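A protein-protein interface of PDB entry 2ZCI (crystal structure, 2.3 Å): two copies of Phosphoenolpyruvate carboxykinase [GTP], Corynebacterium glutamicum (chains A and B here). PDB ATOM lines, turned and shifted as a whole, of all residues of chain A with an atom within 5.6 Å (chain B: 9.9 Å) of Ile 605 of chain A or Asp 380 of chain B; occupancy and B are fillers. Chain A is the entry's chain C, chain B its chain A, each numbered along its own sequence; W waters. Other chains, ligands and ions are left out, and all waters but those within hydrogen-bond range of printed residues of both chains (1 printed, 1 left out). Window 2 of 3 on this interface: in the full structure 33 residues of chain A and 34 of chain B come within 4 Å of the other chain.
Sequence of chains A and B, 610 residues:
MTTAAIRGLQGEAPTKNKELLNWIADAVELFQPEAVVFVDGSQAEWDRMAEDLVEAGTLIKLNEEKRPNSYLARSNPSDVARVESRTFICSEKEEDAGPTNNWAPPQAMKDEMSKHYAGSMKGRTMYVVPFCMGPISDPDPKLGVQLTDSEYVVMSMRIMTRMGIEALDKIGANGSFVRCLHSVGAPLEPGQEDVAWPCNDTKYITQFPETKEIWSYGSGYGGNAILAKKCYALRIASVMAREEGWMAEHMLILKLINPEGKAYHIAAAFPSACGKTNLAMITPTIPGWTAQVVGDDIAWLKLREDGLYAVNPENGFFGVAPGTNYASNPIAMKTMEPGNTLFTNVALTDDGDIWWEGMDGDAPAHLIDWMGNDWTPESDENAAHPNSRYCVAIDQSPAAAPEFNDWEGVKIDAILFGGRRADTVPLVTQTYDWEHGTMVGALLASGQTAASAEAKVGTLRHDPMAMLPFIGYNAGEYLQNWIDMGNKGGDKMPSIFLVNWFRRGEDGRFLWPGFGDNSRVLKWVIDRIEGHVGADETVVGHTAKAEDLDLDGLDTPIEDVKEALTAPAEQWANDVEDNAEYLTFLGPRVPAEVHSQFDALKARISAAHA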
ATOM      1  N   VAL A 539       8.678   7.020   1.210  1.00  0.00           N
ATOM      2  CA  VAL A 539      10.110   6.525   1.285  1.00  0.00           C
ATOM      3  C   VAL A 539      10.118   4.995   1.300  1.00  0.00           C
ATOM      4  O   VAL A 539      11.019   4.399   0.734  1.00  0.00           O
ATOM      5  CB  VAL A 539      10.910   7.124   2.520  1.00  0.00           C
ATOM      6  CG1 VAL A 539      11.070   8.614   2.359  1.00  0.00           C
ATOM      7  CG2 VAL A 539      10.205   6.751   3.916  1.00  0.00           C
ATOM      8  N   ALA A 569       9.097  11.247   7.296  1.00  0.00           N
ATOM      9  CA  ALA A 569      10.468  10.966   6.869  1.00  0.00           C
ATOM     10  C   ALA A 569      11.471  11.212   7.949  1.00  0.00           C
ATOM     11  O   ALA A 569      12.527  10.580   7.933  1.00  0.00           O
ATOM     12  CB  ALA A 569      10.810  11.755   5.678  1.00  0.00           C
ATOM     13  N   GLU A 570      11.138  12.113   8.857  1.00  0.00           N
ATOM     14  CA  GLU A 570      11.796  12.259  10.158  1.00  0.00           C
ATOM     15  C   GLU A 570      11.858  10.957  10.998  1.00  0.00           C
ATOM     16  O   GLU A 570      12.874  10.619  11.588  1.00  0.00           O
ATOM     17  CB  GLU A 570      11.053  13.268  10.982  1.00  0.00           C
ATOM     18  CG  GLU A 570      10.558  14.517  10.258  1.00  0.00           C
ATOM     19  CD  GLU A 570      10.593  15.736  11.202  1.00  0.00           C
ATOM     20  OE1 GLU A 570      10.720  15.432  12.429  1.00  0.00           O
ATOM     21  OE2 GLU A 570      10.494  16.953  10.750  1.00  0.00           O
ATOM     22  N   TRP A 572      11.565   7.906   9.651  1.00  0.00           N
ATOM     23  CA  TRP A 572      12.458   7.075   8.887  1.00  0.00           C
ATOM     24  C   TRP A 572      13.964   7.474   9.081  1.00  0.00           C
ATOM     25  O   TRP A 572      14.817   6.591   9.156  1.00  0.00           O
ATOM     26  CB  TRP A 572      11.968   6.998   7.396  1.00  0.00           C
ATOM     27  CG  TRP A 572      10.856   6.028   7.267  1.00  0.00           C
ATOM     28  CD1 TRP A 572       9.488   6.281   7.470  1.00  0.00           C
ATOM     29  CD2 TRP A 572      10.973   4.608   7.031  1.00  0.00           C
ATOM     30  NE1 TRP A 572       8.784   5.106   7.378  1.00  0.00           N
ATOM     31  CE2 TRP A 572       9.650   4.068   7.082  1.00  0.00           C
ATOM     32  CE3 TRP A 572      12.055   3.747   6.791  1.00  0.00           C
ATOM     33  CZ2 TRP A 572       9.392   2.723   6.938  1.00  0.00           C
ATOM     34  CZ3 TRP A 572      11.819   2.379   6.596  1.00  0.00           C
ATOM     35  CH2 TRP A 572      10.477   1.884   6.692  1.00  0.00           C
ATOM     36  N   ALA A 573      14.286   8.787   9.058  1.00  0.00           N
ATOM     37  CA  ALA A 573      15.602   9.374   9.416  1.00  0.00           C
ATOM     38  C   ALA A 573      16.053   8.872  10.789  1.00  0.00           C
ATOM     39  O   ALA A 573      17.148   8.468  10.954  1.00  0.00           O
ATOM     40  CB  ALA A 573      15.515  10.905   9.456  1.00  0.00           C
ATOM     41  N   VAL A 576      17.635   5.288  10.628  1.00  0.00           N
ATOM     42  CA  VAL A 576      18.652   5.032   9.590  1.00  0.00           C
ATOM     43  C   VAL A 576      19.899   4.410  10.222  1.00  0.00           C
ATOM     44  O   VAL A 576      20.368   3.341   9.822  1.00  0.00           O
ATOM     45  CB  VAL A 576      18.999   6.331   8.747  1.00  0.00           C
ATOM     46  CG1 VAL A 576      20.435   6.232   8.027  1.00  0.00           C
ATOM     47  CG2 VAL A 576      17.929   6.684   7.747  1.00  0.00           C
ATOM     48  N   GLU A 577      20.409   5.033  11.253  1.00  0.00           N
ATOM     49  CA  GLU A 577      21.628   4.520  11.949  1.00  0.00           C
ATOM     50  C   GLU A 577      21.461   3.107  12.487  1.00  0.00           C
ATOM     51  O   GLU A 577      22.367   2.349  12.425  1.00  0.00           O
ATOM     52  CB  GLU A 577      22.036   5.476  13.105  1.00  0.00           C
ATOM     53  CG  GLU A 577      23.443   5.076  13.891  1.00  0.00           C
ATOM     54  CD  GLU A 577      24.725   4.936  12.980  1.00  0.00           C
ATOM     55  OE1 GLU A 577      25.567   4.017  13.206  1.00  0.00           O
ATOM     56  OE2 GLU A 577      24.942   5.744  12.031  1.00  0.00           O
ATOM     57  N   ALA A 600      19.692   3.406  -1.363  1.00  0.00           N
ATOM     58  CA  ALA A 600      18.545   3.979  -2.030  1.00  0.00           C
ATOM     59  C   ALA A 600      17.470   4.457  -1.113  1.00  0.00           C
ATOM     60  O   ALA A 600      16.878   5.546  -1.325  1.00  0.00           O
ATOM     61  CB  ALA A 600      17.994   3.007  -3.134  1.00  0.00           C
ATOM     62  N   LEU A 601      17.222   3.652  -0.088  1.00  0.00           N
ATOM     63  CA  LEU A 601      16.343   4.010   1.035  1.00  0.00           C
ATOM     64  C   LEU A 601      16.799   5.274   1.767  1.00  0.00           C
ATOM     65  O   LEU A 601      15.998   6.120   2.116  1.00  0.00           O
ATOM     66  CB  LEU A 601      16.278   2.860   2.065  1.00  0.00           C
ATOM     67  CG  LEU A 601      15.355   3.212   3.266  1.00  0.00           C
ATOM     68  CD1 LEU A 601      14.003   3.800   2.833  1.00  0.00           C
ATOM     69  CD2 LEU A 601      15.180   2.078   4.261  1.00  0.00           C
ATOM     70  N   LYS A 602      18.078   5.329   2.062  1.00  0.00           N
ATOM     71  CA  LYS A 602      18.662   6.514   2.639  1.00  0.00           C
ATOM     72  C   LYS A 602      18.648   7.688   1.626  1.00  0.00           C
ATOM     73  O   LYS A 602      18.316   8.767   2.056  1.00  0.00           O
ATOM     74  CB  LYS A 602      20.093   6.228   3.085  1.00  0.00           C
ATOM     75  CG  LYS A 602      20.239   5.256   4.282  1.00  0.00           C
ATOM     76  CD  LYS A 602      21.762   4.686   4.314  1.00  0.00           C
ATOM     77  CE  LYS A 602      22.893   5.650   4.295  1.00  0.00           C
ATOM     78  NZ  LYS A 602      24.283   5.050   4.030  1.00  0.00           N
ATOM     79  N   ALA A 603      18.969   7.472   0.327  1.00  0.00           N
ATOM     80  CA  ALA A 603      18.799   8.557  -0.682  1.00  0.00           C
ATOM     81  C   ALA A 603      17.378   9.083  -0.648  1.00  0.00           C
ATOM     82  O   ALA A 603      17.194  10.272  -0.630  1.00  0.00           O
ATOM     83  CB  ALA A 603      19.221   8.160  -2.107  1.00  0.00           C
ATOM     84  N   ARG A 604      16.394   8.184  -0.480  1.00  0.00           N
ATOM     85  CA  ARG A 604      15.020   8.529  -0.534  1.00  0.00           C
ATOM     86  C   ARG A 604      14.535   9.318   0.637  1.00  0.00           C
ATOM     87  O   ARG A 604      13.639  10.217   0.449  1.00  0.00           O
ATOM     88  CB  ARG A 604      14.192   7.232  -0.581  1.00  0.00           C
ATOM     89  CG  ARG A 604      13.953   6.629  -1.966  1.00  0.00           C
ATOM     90  CD  ARG A 604      12.744   5.700  -1.851  1.00  0.00           C
ATOM     91  NE  ARG A 604      12.947   4.490  -1.052  1.00  0.00           N
ATOM     92  CZ  ARG A 604      13.556   3.358  -1.472  1.00  0.00           C
ATOM     93  NH1 ARG A 604      14.153   3.254  -2.693  1.00  0.00           N
ATOM     94  NH2 ARG A 604      13.642   2.332  -0.620  1.00  0.00           N
ATOM     95  N   ILE A 605      14.991   8.942   1.868  1.00  0.00           N
ATOM     96  CA  ILE A 605      14.629   9.711   3.102  1.00  0.00           C
ATOM     97  C   ILE A 605      15.329  11.094   3.074  1.00  0.00           C
ATOM     98  O   ILE A 605      14.763  12.140   3.411  1.00  0.00           O
ATOM     99  CB  ILE A 605      15.066   8.957   4.442  1.00  0.00           C
ATOM    100  CG1 ILE A 605      14.268   7.669   4.692  1.00  0.00           C
ATOM    101  CG2 ILE A 605      15.023   9.902   5.627  1.00  0.00           C
ATOM    102  CD1 ILE A 605      15.134   6.508   5.305  1.00  0.00           C
ATOM    103  N   SER A 606      16.605  11.067   2.686  1.00  0.00           N
ATOM    104  CA  SER A 606      17.369  12.306   2.617  1.00  0.00           C
ATOM    105  C   SER A 606      16.645  13.256   1.632  1.00  0.00           C
ATOM    106  O   SER A 606      16.261  14.323   2.129  1.00  0.00           O
ATOM    107  CB  SER A 606      18.817  12.022   2.181  1.00  0.00           C
ATOM    108  OG  SER A 606      19.728  12.882   2.839  1.00  0.00           O
ATOM    109  N   GLU B 357      27.778  13.472  18.536  1.00  0.00           N
ATOM    110  CA  GLU B 357      26.374  13.832  18.779  1.00  0.00           C
ATOM    111  C   GLU B 357      26.183  14.059  20.297  1.00  0.00           C
ATOM    112  O   GLU B 357      26.804  13.346  21.113  1.00  0.00           O
ATOM    113  CB  GLU B 357      25.422  12.720  18.289  1.00  0.00           C
ATOM    114  CG  GLU B 357      25.057  12.728  16.731  1.00  0.00           C
ATOM    115  CD  GLU B 357      26.193  12.252  15.823  1.00  0.00           C
ATOM    116  OE1 GLU B 357      27.049  11.447  16.306  1.00  0.00           O
ATOM    117  OE2 GLU B 357      26.207  12.683  14.622  1.00  0.00           O
ATOM    118  N   ASP B 369      33.260  11.554   9.503  1.00  0.00           N
ATOM    119  CA  ASP B 369      32.668  10.640  10.408  1.00  0.00           C
ATOM    120  C   ASP B 369      33.648   9.483  10.740  1.00  0.00           C
ATOM    121  O   ASP B 369      34.715   9.343  10.114  1.00  0.00           O
ATOM    122  CB  ASP B 369      31.288  10.174   9.865  1.00  0.00           C
ATOM    123  CG  ASP B 369      31.396   9.230   8.691  1.00  0.00           C
ATOM    124  OD1 ASP B 369      32.461   8.608   8.477  1.00  0.00           O
ATOM    125  OD2 ASP B 369      30.395   9.032   7.979  1.00  0.00           O
ATOM    126  N   ASP B 374      32.813  12.287   4.687  1.00  0.00           N
ATOM    127  CA  ASP B 374      32.371  13.632   5.026  1.00  0.00           C
ATOM    128  C   ASP B 374      30.924  13.546   5.457  1.00  0.00           C
ATOM    129  O   ASP B 374      30.142  12.806   4.866  1.00  0.00           O
ATOM    130  CB  ASP B 374      32.459  14.454   3.764  1.00  0.00           C
ATOM    131  CG  ASP B 374      33.849  14.475   3.196  1.00  0.00           C
ATOM    132  OD1 ASP B 374      34.847  14.802   3.890  1.00  0.00           O
ATOM    133  OD2 ASP B 374      33.926  14.161   2.005  1.00  0.00           O
ATOM    134  N   TRP B 375      30.597  14.282   6.512  1.00  0.00           N
ATOM    135  CA  TRP B 375      29.326  14.286   7.138  1.00  0.00           C
ATOM    136  C   TRP B 375      28.862  15.734   7.235  1.00  0.00           C
ATOM    137  O   TRP B 375      29.656  16.579   7.608  1.00  0.00           O
ATOM    138  CB  TRP B 375      29.549  13.810   8.552  1.00  0.00           C
ATOM    139  CG  TRP B 375      28.265  13.742   9.453  1.00  0.00           C
ATOM    140  CD1 TRP B 375      27.495  12.655   9.662  1.00  0.00           C
ATOM    141  CD2 TRP B 375      27.665  14.825  10.220  1.00  0.00           C
ATOM    142  NE1 TRP B 375      26.500  12.959  10.484  1.00  0.00           N
ATOM    143  CE2 TRP B 375      26.571  14.276  10.876  1.00  0.00           C
ATOM    144  CE3 TRP B 375      27.982  16.194  10.423  1.00  0.00           C
ATOM    145  CZ2 TRP B 375      25.724  15.031  11.717  1.00  0.00           C
ATOM    146  CZ3 TRP B 375      27.189  16.928  11.284  1.00  0.00           C
ATOM    147  CH2 TRP B 375      26.061  16.333  11.938  1.00  0.00           C
ATOM    148  N   THR B 376      27.569  15.978   7.016  1.00  0.00           N
ATOM    149  CA  THR B 376      26.891  17.283   7.108  1.00  0.00           C
ATOM    150  C   THR B 376      25.797  17.136   8.182  1.00  0.00           C
ATOM    151  O   THR B 376      25.288  16.007   8.356  1.00  0.00           O
ATOM    152  CB  THR B 376      26.193  17.572   5.658  1.00  0.00           C
ATOM    153  OG1 THR B 376      25.044  18.407   5.812  1.00  0.00           O
ATOM    154  CG2 THR B 376      25.689  16.220   4.990  1.00  0.00           C
ATOM    155  N   PRO B 377      25.342  18.221   8.860  1.00  0.00           N
ATOM    156  CA  PRO B 377      24.060  17.945   9.586  1.00  0.00           C
ATOM    157  C   PRO B 377      22.791  17.613   8.780  1.00  0.00           C
ATOM    158  O   PRO B 377      21.736  17.584   9.378  1.00  0.00           O
ATOM    159  CB  PRO B 377      23.806  19.233  10.415  1.00  0.00           C
ATOM    160  CG  PRO B 377      25.050  19.891  10.450  1.00  0.00           C
ATOM    161  CD  PRO B 377      25.734  19.613   9.110  1.00  0.00           C
ATOM    162  N   GLU B 378      22.916  17.333   7.473  1.00  0.00           N
ATOM    163  CA  GLU B 378      21.884  16.656   6.635  1.00  0.00           C
ATOM    164  C   GLU B 378      21.895  15.150   6.734  1.00  0.00           C
ATOM    165  O   GLU B 378      20.840  14.570   6.475  1.00  0.00           O
ATOM    166  CB  GLU B 378      22.052  16.969   5.123  1.00  0.00           C
ATOM    167  CG  GLU B 378      20.977  17.952   4.536  1.00  0.00           C
ATOM    168  CD  GLU B 378      21.523  18.779   3.354  1.00  0.00           C
ATOM    169  OE1 GLU B 378      21.281  20.023   3.353  1.00  0.00           O
ATOM    170  OE2 GLU B 378      22.190  18.199   2.425  1.00  0.00           O
ATOM    171  N   SER B 379      23.066  14.520   7.014  1.00  0.00           N
ATOM    172  CA  SER B 379      23.210  13.030   7.034  1.00  0.00           C
ATOM    173  C   SER B 379      22.218  12.534   8.077  1.00  0.00           C
ATOM    174  O   SER B 379      21.830  13.330   8.978  1.00  0.00           O
ATOM    175  CB  SER B 379      24.578  12.510   7.471  1.00  0.00           C
ATOM    176  OG  SER B 379      25.483  13.580   7.503  1.00  0.00           O
ATOM    177  N   ASP B 380      21.782  11.270   7.912  1.00  0.00           N
ATOM    178  CA  ASP B 380      20.786  10.732   8.815  1.00  0.00           C
ATOM    179  C   ASP B 380      21.442   9.749   9.714  1.00  0.00           C
ATOM    180  O   ASP B 380      20.768   9.186  10.626  1.00  0.00           O
ATOM    181  CB  ASP B 380      19.673  10.066   8.080  1.00  0.00           C
ATOM    182  CG  ASP B 380      18.734  11.048   7.536  1.00  0.00           C
ATOM    183  OD1 ASP B 380      18.507  12.057   8.288  1.00  0.00           O
ATOM    184  OD2 ASP B 380      18.289  10.838   6.351  1.00  0.00           O
ATOM    185  N   GLU B 381      22.760   9.620   9.435  1.00  0.00           N
ATOM    186  CA  GLU B 381      23.743   8.774  10.044  1.00  0.00           C
ATOM    187  C   GLU B 381      24.640   9.513  10.984  1.00  0.00           C
ATOM    188  O   GLU B 381      25.100  10.610  10.662  1.00  0.00           O
ATOM    189  CB  GLU B 381      24.635   8.282   8.960  1.00  0.00           C
ATOM    190  CG  GLU B 381      23.841   7.306   8.149  1.00  0.00           C
ATOM    191  CD  GLU B 381      24.599   6.692   7.071  1.00  0.00           C
ATOM    192  OE1 GLU B 381      24.575   7.381   6.003  1.00  0.00           O
ATOM    193  OE2 GLU B 381      25.140   5.531   7.301  1.00  0.00           O
ATOM    194  N   ASN B 382      24.878   8.902  12.144  1.00  0.00           N
ATOM    195  CA  ASN B 382      25.720   9.447  13.173  1.00  0.00           C
ATOM    196  C   ASN B 382      27.159   9.719  12.687  1.00  0.00           C
ATOM    197  O   ASN B 382      27.711   8.905  12.069  1.00  0.00           O
ATOM    198  CB  ASN B 382      25.687   8.507  14.378  1.00  0.00           C
ATOM    199  CG  ASN B 382      24.349   8.614  15.159  1.00  0.00           C
ATOM    200  OD1 ASN B 382      23.291   8.954  14.601  1.00  0.00           O
ATOM    201  ND2 ASN B 382      24.399   8.370  16.450  1.00  0.00           N
ATOM    202  N   ALA B 383      27.728  10.875  13.033  1.00  0.00           N
ATOM    203  CA  ALA B 383      29.161  11.164  12.876  1.00  0.00           C
ATOM    204  C   ALA B 383      30.053  10.337  13.811  1.00  0.00           C
ATOM    205  O   ALA B 383      31.122   9.894  13.402  1.00  0.00           O
ATOM    206  CB  ALA B 383      29.400  12.635  13.123  1.00  0.00           C
ATOM    207  N   ALA B 384      29.612  10.127  15.063  1.00  0.00           N
ATOM    208  CA  ALA B 384      30.361   9.368  16.033  1.00  0.00           C
ATOM    209  C   ALA B 384      29.609   8.045  16.098  1.00  0.00           C
ATOM    210  O   ALA B 384      28.408   8.054  16.096  1.00  0.00           O
ATOM    211  CB  ALA B 384      30.303  10.040  17.387  1.00  0.00           C
ATOM    212  N   PRO B 386      27.639   5.365  17.873  1.00  0.00           N
ATOM    213  CA  PRO B 386      27.020   5.426  19.207  1.00  0.00           C
ATOM    214  C   PRO B 386      27.742   4.662  20.335  1.00  0.00           C
ATOM    215  O   PRO B 386      27.547   4.942  21.484  1.00  0.00           O
ATOM    216  CB  PRO B 386      25.656   4.780  18.970  1.00  0.00           C
ATOM    217  CG  PRO B 386      25.405   5.024  17.545  1.00  0.00           C
ATOM    218  CD  PRO B 386      26.748   4.696  16.939  1.00  0.00           C
HETATM  219  O   HOH W   1      19.380   7.725  12.185  1.00  0.00           O
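The backbone NH (N) of Asn 382 of chain B sits at hydrogen-bond distance from the side-chain carboxylate (OE2) of Glu 577 of chain A (3.2 Å).
The side-chain carboxylate (OE1) of Glu 381 of chain B lies within salt-bridge range of the side-chain amino group (NZ) of Lys 602 of chain A, at 3.1 Å.
NE1 of Trp 375 of chain B sits at hydrogen-bond distance from O of Glu 381 of chain B (2.7 Å).
Among the printed residues, pairs that only touch across the chains: Ala 573 of chain A with Asp 380 of chain B (3.4 Å), Val 576 of chain A with Asp 380 of chain B (3.8 Å), Val 576 of chain A with Glu 381 of chain B (3.6 Å), Glu 577 of chain A with Glu 381 of chain B (3.8 Å), Glu 577 of chain A with Pro 386 of chain B (3.97 Å) and Ile 605 of chain A with Asp 380 of chain B (3.5 Å).
Ala 569 of chain A touches none of the printed residues of chain B.
Ala 573 of chain A touches one residue of chain B.
Of the printed residues of chain B, Val 576 of chain A touches Asp 380 (3.8 Å) and Glu 381 (3.6 Å).
Of the printed residues of chain B, Glu 577 of chain A touches Glu 381 (3.8 Å), Asn 382 (3.2 Å) and Pro 386 (3.97 Å).
Printed residues of chain B within 4 Å of Lys 602 of chain A: Glu 381.
No residue of chain B comes within 4 Å of Ser 606 of chain A.
Thr 376 of chain B touches none of the printed residues of chain A.
Of chain A, only Ala 573 (3.4 Å), Val 576 (3.8 Å) and Ile 605 (3.5 Å) come within 4 Å of Asp 380 of chain B.
Printed residues of chain A within 4 Å of Asn 382 of chain B: Glu 577.
Printed residues of chain A within 4 Å of Pro 386 of chain B: Glu 577 (3.97 Å).
The nearest residue of chain B that does not touch Ile 605 of chain A is Glu 378 of chain B (7.2 Å).
Hydrophobic or aromatic side chains of chain B within 4 Å of the printed part of chain A: Pro 386.
Along chain B the printed residues that touch a printed residue of chain A span positions 380 to 386.
Of the 14 printed residues of chain A, 5 touch a printed residue of chain B.
Printed residues of chain A that touch a printed residue of chain B: Ala 573, Val 576, Glu 577, Lys 602 and Ile 605.
Among the printed residues, 8 pairs touch across the chains.
No position is printed for both chains.
Of the 8 pairs that touch across the chains among the printed residues, none has its exchanged pair printed and touching as well.
Water W1 lies within hydrogen-bond range of O of Asp 380 of chain B (2.5 Å), O of Ala 573 of chain A (2.7 Å), N of Glu 577 of chain A (3.0 Å) and N of Val 576 of chain A (3.4 Å).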
